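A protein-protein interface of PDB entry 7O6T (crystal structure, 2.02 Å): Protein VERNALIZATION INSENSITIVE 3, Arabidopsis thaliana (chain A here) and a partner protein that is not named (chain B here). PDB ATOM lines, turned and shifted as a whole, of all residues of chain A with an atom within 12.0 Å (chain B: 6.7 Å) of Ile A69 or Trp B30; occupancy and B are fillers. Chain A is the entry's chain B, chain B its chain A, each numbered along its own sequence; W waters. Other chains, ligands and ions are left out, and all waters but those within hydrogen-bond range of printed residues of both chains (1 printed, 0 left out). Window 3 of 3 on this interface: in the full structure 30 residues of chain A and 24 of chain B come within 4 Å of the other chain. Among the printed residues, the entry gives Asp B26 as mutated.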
ATOM      1  N   LEU A  57     -25.615  -6.944 -40.789  1.00  0.00           N
ATOM      2  CA  LEU A  57     -25.975  -7.287 -39.412  1.00  0.00           C
ATOM      3  C   LEU A  57     -25.205  -8.543 -38.942  1.00  0.00           C
ATOM      4  O   LEU A  57     -24.603  -8.557 -37.877  1.00  0.00           O
ATOM      5  CB  LEU A  57     -27.498  -7.505 -39.300  1.00  0.00           C
ATOM      6  CG  LEU A  57     -28.055  -8.194 -38.037  1.00  0.00           C
ATOM      7  CD1 LEU A  57     -27.749  -7.346 -36.827  1.00  0.00           C
ATOM      8  CD2 LEU A  57     -29.556  -8.434 -38.124  1.00  0.00           C
ATOM      9  N   GLY A  58     -25.254  -9.600 -39.750  1.00  0.00           N
ATOM     10  CA  GLY A  58     -24.483 -10.805 -39.514  1.00  0.00           C
ATOM     11  C   GLY A  58     -23.012 -10.496 -39.229  1.00  0.00           C
ATOM     12  O   GLY A  58     -22.467 -10.980 -38.256  1.00  0.00           O
ATOM     13  N   GLN A  59     -22.380  -9.691 -40.094  1.00  0.00           N
ATOM     14  CA  GLN A  59     -20.986  -9.299 -39.935  1.00  0.00           C
ATOM     15  C   GLN A  59     -20.769  -8.557 -38.627  1.00  0.00           C
ATOM     16  O   GLN A  59     -19.836  -8.850 -37.904  1.00  0.00           O
ATOM     17  CB  GLN A  59     -20.499  -8.444 -41.103  1.00  0.00           C
ATOM     18  CG  GLN A  59     -18.971  -8.417 -41.189  1.00  0.00           C
ATOM     19  CD  GLN A  59     -18.380  -9.825 -41.277  1.00  0.00           C
ATOM     20  OE1 GLN A  59     -18.668 -10.552 -42.231  1.00  0.00           O
ATOM     21  NE2 GLN A  59     -17.574 -10.233 -40.266  1.00  0.00           N
ATOM     22  N   GLN A  60     -21.648  -7.605 -38.320  1.00  0.00           N
ATOM     23  CA  GLN A  60     -21.557  -6.844 -37.087  1.00  0.00           C
ATOM     24  C   GLN A  60     -21.666  -7.739 -35.851  1.00  0.00           C
ATOM     25  O   GLN A  60     -20.918  -7.558 -34.906  1.00  0.00           O
ATOM     26  CB  GLN A  60     -22.573  -5.693 -37.063  1.00  0.00           C
ATOM     27  CG  GLN A  60     -22.282  -4.655 -38.158  1.00  0.00           C
ATOM     28  CD  GLN A  60     -22.993  -3.318 -37.974  1.00  0.00           C
ATOM     29  OE1 GLN A  60     -22.759  -2.621 -36.987  1.00  0.00           O
ATOM     30  NE2 GLN A  60     -23.825  -2.929 -38.951  1.00  0.00           N
ATOM     31  N   LEU A  61     -22.591  -8.704 -35.859  1.00  0.00           N
ATOM     32  CA  LEU A  61     -22.761  -9.612 -34.725  1.00  0.00           C
ATOM     33  C   LEU A  61     -21.534 -10.493 -34.560  1.00  0.00           C
ATOM     34  O   LEU A  61     -21.085 -10.719 -33.446  1.00  0.00           O
ATOM     35  CB  LEU A  61     -23.992 -10.518 -34.873  1.00  0.00           C
ATOM     36  CG  LEU A  61     -25.368  -9.885 -34.849  1.00  0.00           C
ATOM     37  CD1 LEU A  61     -26.375 -11.013 -34.699  1.00  0.00           C
ATOM     38  CD2 LEU A  61     -25.513  -8.891 -33.714  1.00  0.00           C
ATOM     39  N   VAL A  62     -21.026 -11.010 -35.685  1.00  0.00           N
ATOM     40  CA  VAL A  62     -19.839 -11.849 -35.705  1.00  0.00           C
ATOM     41  C   VAL A  62     -18.640 -11.034 -35.222  1.00  0.00           C
ATOM     42  O   VAL A  62     -17.890 -11.511 -34.395  1.00  0.00           O
ATOM     43  CB  VAL A  62     -19.590 -12.465 -37.101  1.00  0.00           C
ATOM     44  CG1 VAL A  62     -18.208 -13.108 -37.184  1.00  0.00           C
ATOM     45  CG2 VAL A  62     -20.675 -13.488 -37.446  1.00  0.00           C
ATOM     46  N   ASP A  63     -18.499  -9.790 -35.701  1.00  0.00           N
ATOM     47  CA  ASP A  63     -17.413  -8.898 -35.271  1.00  0.00           C
ATOM     48  C   ASP A  63     -17.487  -8.583 -33.780  1.00  0.00           C
ATOM     49  O   ASP A  63     -16.463  -8.615 -33.105  1.00  0.00           O
ATOM     50  CB  ASP A  63     -17.380  -7.580 -36.064  1.00  0.00           C
ATOM     51  CG  ASP A  63     -16.867  -7.743 -37.478  1.00  0.00           C
ATOM     52  OD1 ASP A  63     -16.431  -8.857 -37.848  1.00  0.00           O
ATOM     53  OD2 ASP A  63     -16.928  -6.731 -38.229  1.00  0.00           O
ATOM     54  N   THR A  64     -18.688  -8.277 -33.279  1.00  0.00           N
ATOM     55  CA  THR A  64     -18.899  -7.990 -31.859  1.00  0.00           C
ATOM     56  C   THR A  64     -18.515  -9.166 -30.976  1.00  0.00           C
ATOM     57  O   THR A  64     -17.807  -9.003 -29.987  1.00  0.00           O
ATOM     58  CB  THR A  64     -20.375  -7.639 -31.576  1.00  0.00           C
ATOM     59  OG1 THR A  64     -20.775  -6.561 -32.409  1.00  0.00           O
ATOM     60  CG2 THR A  64     -20.586  -7.256 -30.122  1.00  0.00           C
ATOM     61  N   PHE A  65     -19.000 -10.359 -31.343  1.00  0.00           N
ATOM     62  CA  PHE A  65     -18.680 -11.615 -30.665  1.00  0.00           C
ATOM     63  C   PHE A  65     -17.180 -11.851 -30.620  1.00  0.00           C
ATOM     64  O   PHE A  65     -16.633 -12.207 -29.556  1.00  0.00           O
ATOM     65  CB  PHE A  65     -19.389 -12.753 -31.418  1.00  0.00           C
ATOM     66  CG  PHE A  65     -19.016 -14.134 -31.017  1.00  0.00           C
ATOM     67  CD1 PHE A  65     -17.921 -14.769 -31.600  1.00  0.00           C
ATOM     68  CD2 PHE A  65     -19.820 -14.868 -30.144  1.00  0.00           C
ATOM     69  CE1 PHE A  65     -17.603 -16.084 -31.276  1.00  0.00           C
ATOM     70  CE2 PHE A  65     -19.516 -16.164 -29.822  1.00  0.00           C
ATOM     71  CZ  PHE A  65     -18.396 -16.786 -30.383  1.00  0.00           C
ATOM     72  N   SER A  66     -16.529 -11.690 -31.778  1.00  0.00           N
ATOM     73  CA  SER A  66     -15.111 -11.984 -31.951  1.00  0.00           C
ATOM     74  C   SER A  66     -14.261 -11.045 -31.122  1.00  0.00           C
ATOM     75  O   SER A  66     -13.300 -11.472 -30.477  1.00  0.00           O
ATOM     76  CB  SER A  66     -14.729 -11.888 -33.422  1.00  0.00           C
ATOM     77  OG  SER A  66     -15.359 -12.954 -34.135  1.00  0.00           O
ATOM     78  N   GLU A  67     -14.640  -9.766 -31.127  1.00  0.00           N
ATOM     79  CA  GLU A  67     -13.923  -8.753 -30.369  1.00  0.00           C
ATOM     80  C   GLU A  67     -14.020  -9.047 -28.900  1.00  0.00           C
ATOM     81  O   GLU A  67     -13.021  -8.933 -28.187  1.00  0.00           O
ATOM     82  CB  GLU A  67     -14.468  -7.359 -30.649  1.00  0.00           C
ATOM     83  CG  GLU A  67     -14.126  -6.858 -32.034  1.00  0.00           C
ATOM     84  CD  GLU A  67     -14.662  -5.463 -32.285  1.00  0.00           C
ATOM     85  OE1 GLU A  67     -14.451  -4.594 -31.403  1.00  0.00           O
ATOM     86  OE2 GLU A  67     -15.280  -5.234 -33.354  1.00  0.00           O
ATOM     87  N   SER A  68     -15.215  -9.441 -28.445  1.00  0.00           N
ATOM     88  CA  SER A  68     -15.431  -9.785 -27.043  1.00  0.00           C
ATOM     89  C   SER A  68     -14.524 -10.914 -26.584  1.00  0.00           C
ATOM     90  O   SER A  68     -13.959 -10.844 -25.509  1.00  0.00           O
ATOM     91  CB  SER A  68     -16.879 -10.160 -26.798  1.00  0.00           C
ATOM     92  OG  SER A  68     -17.129 -10.342 -25.424  1.00  0.00           O
ATOM     93  N   ILE A  69     -14.367 -11.946 -27.419  1.00  0.00           N
ATOM     94  CA  ILE A  69     -13.434 -13.037 -27.124  1.00  0.00           C
ATOM     95  C   ILE A  69     -11.994 -12.535 -27.160  1.00  0.00           C
ATOM     96  O   ILE A  69     -11.204 -12.792 -26.242  1.00  0.00           O
ATOM     97  CB  ILE A  69     -13.522 -14.189 -28.154  1.00  0.00           C
ATOM     98  CG1 ILE A  69     -14.926 -14.798 -28.221  1.00  0.00           C
ATOM     99  CG2 ILE A  69     -12.489 -15.252 -27.808  1.00  0.00           C
ATOM    100  CD1 ILE A  69     -15.587 -14.961 -26.879  1.00  0.00           C
ATOM    101  N   LEU A  70     -11.694 -11.822 -28.256  1.00  0.00           N
ATOM    102  CA  LEU A  70     -10.370 -11.418 -28.740  1.00  0.00           C
ATOM    103  C   LEU A  70      -9.898 -12.405 -29.840  1.00  0.00           C
ATOM    104  O   LEU A  70     -10.685 -12.925 -30.642  1.00  0.00           O
ATOM    105  CB  LEU A  70      -9.338 -11.220 -27.603  1.00  0.00           C
ATOM    106  CG  LEU A  70      -9.421  -9.900 -26.818  1.00  0.00           C
ATOM    107  CD1 LEU A  70     -10.757  -9.631 -26.132  1.00  0.00           C
ATOM    108  CD2 LEU A  70      -8.307  -9.890 -25.788  1.00  0.00           C
ATOM    109  N   GLU B  25     -24.827 -21.499 -31.600  1.00  0.00           N
ATOM    110  CA  GLU B  25     -24.686 -22.065 -30.279  1.00  0.00           C
ATOM    111  C   GLU B  25     -23.700 -21.290 -29.423  1.00  0.00           C
ATOM    112  O   GLU B  25     -23.956 -21.016 -28.242  1.00  0.00           O
ATOM    113  CB  GLU B  25     -24.283 -23.535 -30.383  1.00  0.00           C
ATOM    114  CG  GLU B  25     -25.398 -24.352 -31.016  1.00  0.00           C
ATOM    115  CD  GLU B  25     -25.123 -25.846 -31.057  1.00  0.00           C
ATOM    116  OE1 GLU B  25     -23.972 -26.262 -30.836  1.00  0.00           O
ATOM    117  OE2 GLU B  25     -26.084 -26.595 -31.329  1.00  0.00           O
ATOM    118  N   ASP B  26     -22.554 -20.934 -30.005  1.00  0.00           N
ATOM    119  CA  ASP B  26     -21.548 -20.181 -29.275  1.00  0.00           C
ATOM    120  C   ASP B  26     -22.056 -18.786 -28.925  1.00  0.00           C
ATOM    121  O   ASP B  26     -21.749 -18.259 -27.888  1.00  0.00           O
ATOM    122  CB  ASP B  26     -20.244 -20.117 -30.079  1.00  0.00           C
ATOM    123  CG  ASP B  26     -19.479 -21.445 -30.052  1.00  0.00           C
ATOM    124  OD1 ASP B  26     -19.752 -22.290 -29.165  1.00  0.00           O
ATOM    125  OD2 ASP B  26     -18.588 -21.633 -30.898  1.00  0.00           O
ATOM    126  N   PHE B  27     -22.827 -18.182 -29.829  1.00  0.00           N
ATOM    127  CA  PHE B  27     -23.380 -16.856 -29.623  1.00  0.00           C
ATOM    128  C   PHE B  27     -24.307 -16.816 -28.432  1.00  0.00           C
ATOM    129  O   PHE B  27     -24.217 -15.900 -27.609  1.00  0.00           O
ATOM    130  CB  PHE B  27     -24.121 -16.359 -30.862  1.00  0.00           C
ATOM    131  CG  PHE B  27     -24.794 -15.022 -30.660  1.00  0.00           C
ATOM    132  CD1 PHE B  27     -24.106 -13.853 -30.868  1.00  0.00           C
ATOM    133  CD2 PHE B  27     -26.120 -14.967 -30.223  1.00  0.00           C
ATOM    134  CE1 PHE B  27     -24.718 -12.633 -30.684  1.00  0.00           C
ATOM    135  CE2 PHE B  27     -26.742 -13.751 -30.005  1.00  0.00           C
ATOM    136  CZ  PHE B  27     -26.033 -12.582 -30.241  1.00  0.00           C
ATOM    137  N   LEU B  28     -25.170 -17.831 -28.321  1.00  0.00           N
ATOM    138  CA  LEU B  28     -26.103 -17.969 -27.209  1.00  0.00           C
ATOM    139  C   LEU B  28     -25.332 -18.122 -25.886  1.00  0.00           C
ATOM    140  O   LEU B  28     -25.648 -17.455 -24.890  1.00  0.00           O
ATOM    141  CB  LEU B  28     -27.016 -19.176 -27.416  1.00  0.00           C
ATOM    142  CG  LEU B  28     -27.935 -19.146 -28.641  1.00  0.00           C
ATOM    143  CD1 LEU B  28     -28.625 -20.493 -28.829  1.00  0.00           C
ATOM    144  CD2 LEU B  28     -28.933 -18.022 -28.525  1.00  0.00           C
ATOM    145  N   THR B  29     -24.307 -18.987 -25.891  1.00  0.00           N
ATOM    146  CA  THR B  29     -23.438 -19.149 -24.741  1.00  0.00           C
ATOM    147  C   THR B  29     -22.774 -17.814 -24.345  1.00  0.00           C
ATOM    148  O   THR B  29     -22.815 -17.397 -23.189  1.00  0.00           O
ATOM    149  CB  THR B  29     -22.336 -20.198 -25.005  1.00  0.00           C
ATOM    150  OG1 THR B  29     -22.931 -21.452 -25.307  1.00  0.00           O
ATOM    151  CG2 THR B  29     -21.462 -20.358 -23.774  1.00  0.00           C
ATOM    152  N   TRP B  30     -22.168 -17.150 -25.329  1.00  0.00           N
ATOM    153  CA  TRP B  30     -21.470 -15.896 -25.140  1.00  0.00           C
ATOM    154  C   TRP B  30     -22.395 -14.849 -24.556  1.00  0.00           C
ATOM    155  O   TRP B  30     -22.070 -14.203 -23.555  1.00  0.00           O
ATOM    156  CB  TRP B  30     -20.887 -15.431 -26.463  1.00  0.00           C
ATOM    157  CG  TRP B  30     -20.388 -14.014 -26.458  1.00  0.00           C
ATOM    158  CD1 TRP B  30     -19.196 -13.560 -25.965  1.00  0.00           C
ATOM    159  CD2 TRP B  30     -21.066 -12.867 -26.990  1.00  0.00           C
ATOM    160  NE1 TRP B  30     -19.097 -12.212 -26.153  1.00  0.00           N
ATOM    161  CE2 TRP B  30     -20.222 -11.754 -26.787  1.00  0.00           C
ATOM    162  CE3 TRP B  30     -22.299 -12.678 -27.609  1.00  0.00           C
ATOM    163  CZ2 TRP B  30     -20.574 -10.460 -27.174  1.00  0.00           C
ATOM    164  CZ3 TRP B  30     -22.652 -11.378 -28.014  1.00  0.00           C
ATOM    165  CH2 TRP B  30     -21.787 -10.299 -27.811  1.00  0.00           C
ATOM    166  N   TYR B  31     -23.575 -14.705 -25.163  1.00  0.00           N
ATOM    167  CA  TYR B  31     -24.608 -13.731 -24.738  1.00  0.00           C
ATOM    168  C   TYR B  31     -24.970 -13.941 -23.265  1.00  0.00           C
ATOM    169  O   TYR B  31     -25.021 -12.944 -22.519  1.00  0.00           O
ATOM    170  CB  TYR B  31     -25.863 -13.854 -25.589  1.00  0.00           C
ATOM    171  CG  TYR B  31     -26.899 -12.807 -25.288  1.00  0.00           C
ATOM    172  CD1 TYR B  31     -27.836 -12.976 -24.281  1.00  0.00           C
ATOM    173  CD2 TYR B  31     -26.954 -11.645 -26.035  1.00  0.00           C
ATOM    174  CE1 TYR B  31     -28.804 -12.017 -24.027  1.00  0.00           C
ATOM    175  CE2 TYR B  31     -27.913 -10.679 -25.791  1.00  0.00           C
ATOM    176  CZ  TYR B  31     -28.844 -10.864 -24.791  1.00  0.00           C
ATOM    177  OH  TYR B  31     -29.785  -9.893 -24.591  1.00  0.00           O
ATOM    178  N   SER B  32     -25.243 -15.187 -22.872  1.00  0.00           N
ATOM    179  CA  SER B  32     -25.697 -15.503 -21.531  1.00  0.00           C
ATOM    180  C   SER B  32     -24.600 -15.377 -20.459  1.00  0.00           C
ATOM    181  O   SER B  32     -24.886 -14.934 -19.364  1.00  0.00           O
ATOM    182  CB  SER B  32     -26.303 -16.907 -21.491  1.00  0.00           C
ATOM    183  OG  SER B  32     -25.307 -17.862 -21.763  1.00  0.00           O
ATOM    184  N   LEU B  33     -23.357 -15.736 -20.808  1.00  0.00           N
ATOM    185  CA  LEU B  33     -22.262 -15.880 -19.847  1.00  0.00           C
ATOM    186  C   LEU B  33     -21.057 -14.936 -19.943  1.00  0.00           C
ATOM    187  O   LEU B  33     -20.415 -14.692 -18.946  1.00  0.00           O
ATOM    188  CB  LEU B  33     -21.727 -17.311 -19.904  1.00  0.00           C
ATOM    189  CG  LEU B  33     -22.775 -18.408 -19.648  1.00  0.00           C
ATOM    190  CD1 LEU B  33     -22.130 -19.763 -19.900  1.00  0.00           C
ATOM    191  CD2 LEU B  33     -23.382 -18.347 -18.243  1.00  0.00           C
ATOM    192  N   ARG B  34     -20.740 -14.418 -21.133  1.00  0.00           N
ATOM    193  CA  ARG B  34     -19.490 -13.643 -21.376  1.00  0.00           C
ATOM    194  C   ARG B  34     -19.767 -12.210 -21.853  1.00  0.00           C
ATOM    195  O   ARG B  34     -18.886 -11.355 -21.622  1.00  0.00           O
ATOM    196  CB  ARG B  34     -18.605 -14.344 -22.412  1.00  0.00           C
ATOM    197  CG  ARG B  34     -18.078 -15.703 -21.989  1.00  0.00           C
ATOM    198  CD  ARG B  34     -17.127 -15.643 -20.811  1.00  0.00           C
ATOM    199  NE  ARG B  34     -17.100 -16.928 -20.127  1.00  0.00           N
ATOM    200  CZ  ARG B  34     -16.107 -17.807 -20.183  1.00  0.00           C
ATOM    201  NH1 ARG B  34     -15.015 -17.559 -20.890  1.00  0.00           N
ATOM    202  NH2 ARG B  34     -16.207 -18.944 -19.517  1.00  0.00           N
ATOM    203  N   ALA B  35     -20.898 -11.949 -22.521  1.00  0.00           N
ATOM    204  CA  ALA B  35     -21.135 -10.624 -23.062  1.00  0.00           C
ATOM    205  C   ALA B  35     -21.282  -9.591 -21.937  1.00  0.00           C
ATOM    206  O   ALA B  35     -21.981  -9.822 -20.965  1.00  0.00           O
ATOM    207  CB  ALA B  35     -22.373 -10.613 -23.954  1.00  0.00           C
ATOM    208  N   THR B  36     -20.630  -8.439 -22.101  1.00  0.00           N
ATOM    209  CA  THR B  36     -20.775  -7.323 -21.176  1.00  0.00           C
ATOM    210  C   THR B  36     -22.123  -6.649 -21.393  1.00  0.00           C
ATOM    211  O   THR B  36     -22.811  -6.910 -22.403  1.00  0.00           O
ATOM    212  CB  THR B  36     -19.658  -6.294 -21.362  1.00  0.00           C
ATOM    213  OG1 THR B  36     -19.758  -5.707 -22.653  1.00  0.00           O
ATOM    214  CG2 THR B  36     -18.291  -6.959 -21.214  1.00  0.00           C
ATOM    215  N   GLU B  39     -22.009  -4.842 -24.653  1.00  0.00           N
ATOM    216  CA  GLU B  39     -22.109  -5.747 -25.798  1.00  0.00           C
ATOM    217  C   GLU B  39     -23.550  -6.224 -26.023  1.00  0.00           C
ATOM    218  O   GLU B  39     -23.990  -6.337 -27.149  1.00  0.00           O
ATOM    219  CB  GLU B  39     -21.142  -6.918 -25.641  1.00  0.00           C
ATOM    220  CG  GLU B  39     -19.702  -6.471 -25.795  1.00  0.00           C
ATOM    221  CD  GLU B  39     -18.677  -7.467 -25.288  1.00  0.00           C
ATOM    222  OE1 GLU B  39     -19.010  -8.374 -24.508  1.00  0.00           O
ATOM    223  OE2 GLU B  39     -17.508  -7.303 -25.664  1.00  0.00           O
ATOM    224  N   VAL B  40     -24.264  -6.494 -24.928  1.00  0.00           N
ATOM    225  CA  VAL B  40     -25.662  -6.917 -24.975  1.00  0.00           C
ATOM    226  C   VAL B  40     -26.519  -5.814 -25.582  1.00  0.00           C
ATOM    227  O   VAL B  40     -27.417  -6.053 -26.405  1.00  0.00           O
ATOM    228  CB  VAL B  40     -26.170  -7.290 -23.563  1.00  0.00           C
ATOM    229  CG1 VAL B  40     -27.697  -7.355 -23.516  1.00  0.00           C
ATOM    230  CG2 VAL B  40     -25.550  -8.608 -23.123  1.00  0.00           C
ATOM    231  N   VAL B  43     -25.956  -5.706 -29.320  1.00  0.00           N
ATOM    232  CA  VAL B  43     -26.754  -6.761 -29.941  1.00  0.00           C
ATOM    233  C   VAL B  43     -28.233  -6.374 -30.035  1.00  0.00           C
ATOM    234  O   VAL B  43     -28.841  -6.478 -31.080  1.00  0.00           O
ATOM    235  CB  VAL B  43     -26.584  -8.091 -29.151  1.00  0.00           C
ATOM    236  CG1 VAL B  43     -27.622  -9.122 -29.557  1.00  0.00           C
ATOM    237  CG2 VAL B  43     -25.198  -8.642 -29.363  1.00  0.00           C
HETATM  238  O   HOH W   1     -17.182  -6.441 -28.710  1.00  0.00           O
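The indole nitrogen (NE1) of Trp B30 sits at hydrogen-bond distance from the side-chain hydroxyl (OG) of Ser A68, at 2.8 Å. OG of Ser A68 lies within hydrogen-bond range of OE1 of Glu B39 (2.9 Å).
The backbone NH (N) of Ala B35 sits at hydrogen-bond distance from the backbone carbonyl oxygen (O) of Trp B30. The backbone NH of Thr B36 is in hydrogen-bond range of the side-chain carboxylate of Glu B39 (2.9 Å).
Phe A65 touches Asp B26 (CE2 to O, 3.6 Å). Phe B27 touches Phe A65. CE2 of Phe A65 touches CB of Trp B30 (3.7 Å). CD1 of Ile A69 touches CD1 of Trp B30, 3.98 Å away.
Asp A63 touches none of the printed residues of chain B. Of the printed residues of chain B, Phe A65 touches Asp B26 (3.6 Å), Phe B27 (3.9 Å) and Trp B30 (3.7 Å). Printed residues of chain B within 4 Å of Ser A68: Trp B30 (2.8 Å) and Glu B39 (2.9 Å). Printed residues of chain A within 4 Å of Asp B26: Phe A65 (3.6 Å). Of chain A, only Phe A65 (3.9 Å) comes within 4 Å of Phe B27. No residue of chain A comes within 4 Å of Thr B29. Printed residues of chain A within 4 Å of Trp B30: Phe A65 (3.7 Å), Ser A68 (2.8 Å) and Ile A69 (3.98 Å). No residue of chain A comes within 4 Å of Ser B32. Leu B33 touches none of the printed residues of chain A. No residue of chain A comes within 4 Å of Val B40. Val B43 touches none of the printed residues of chain A. The nearest printed residue of chain A that does not touch Trp B30 is Thr A64 (4.01 Å). The nearest printed residue of chain A that does not touch Asp B26 is Ile A69 (7.1 Å).
Hydrophobic or aromatic side chains of chain B within 4 Å of the printed part of chain A: Trp B30. Along chain B the printed residues that touch a printed residue of chain A span positions 26 to 39. Of the 14 printed residues of chain A, 3 touch a printed residue of chain B. Hydrophobic or aromatic side chains of chain A within 4 Å of the printed part of chain B: Phe A65 and Ile A69. Among the printed residues, no Asp or Glu carboxylate lies within 4 Å of a Lys or Arg side-chain nitrogen of the other chain.
Water W1 bridges O of Thr A64 and OE2 of Glu B39.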
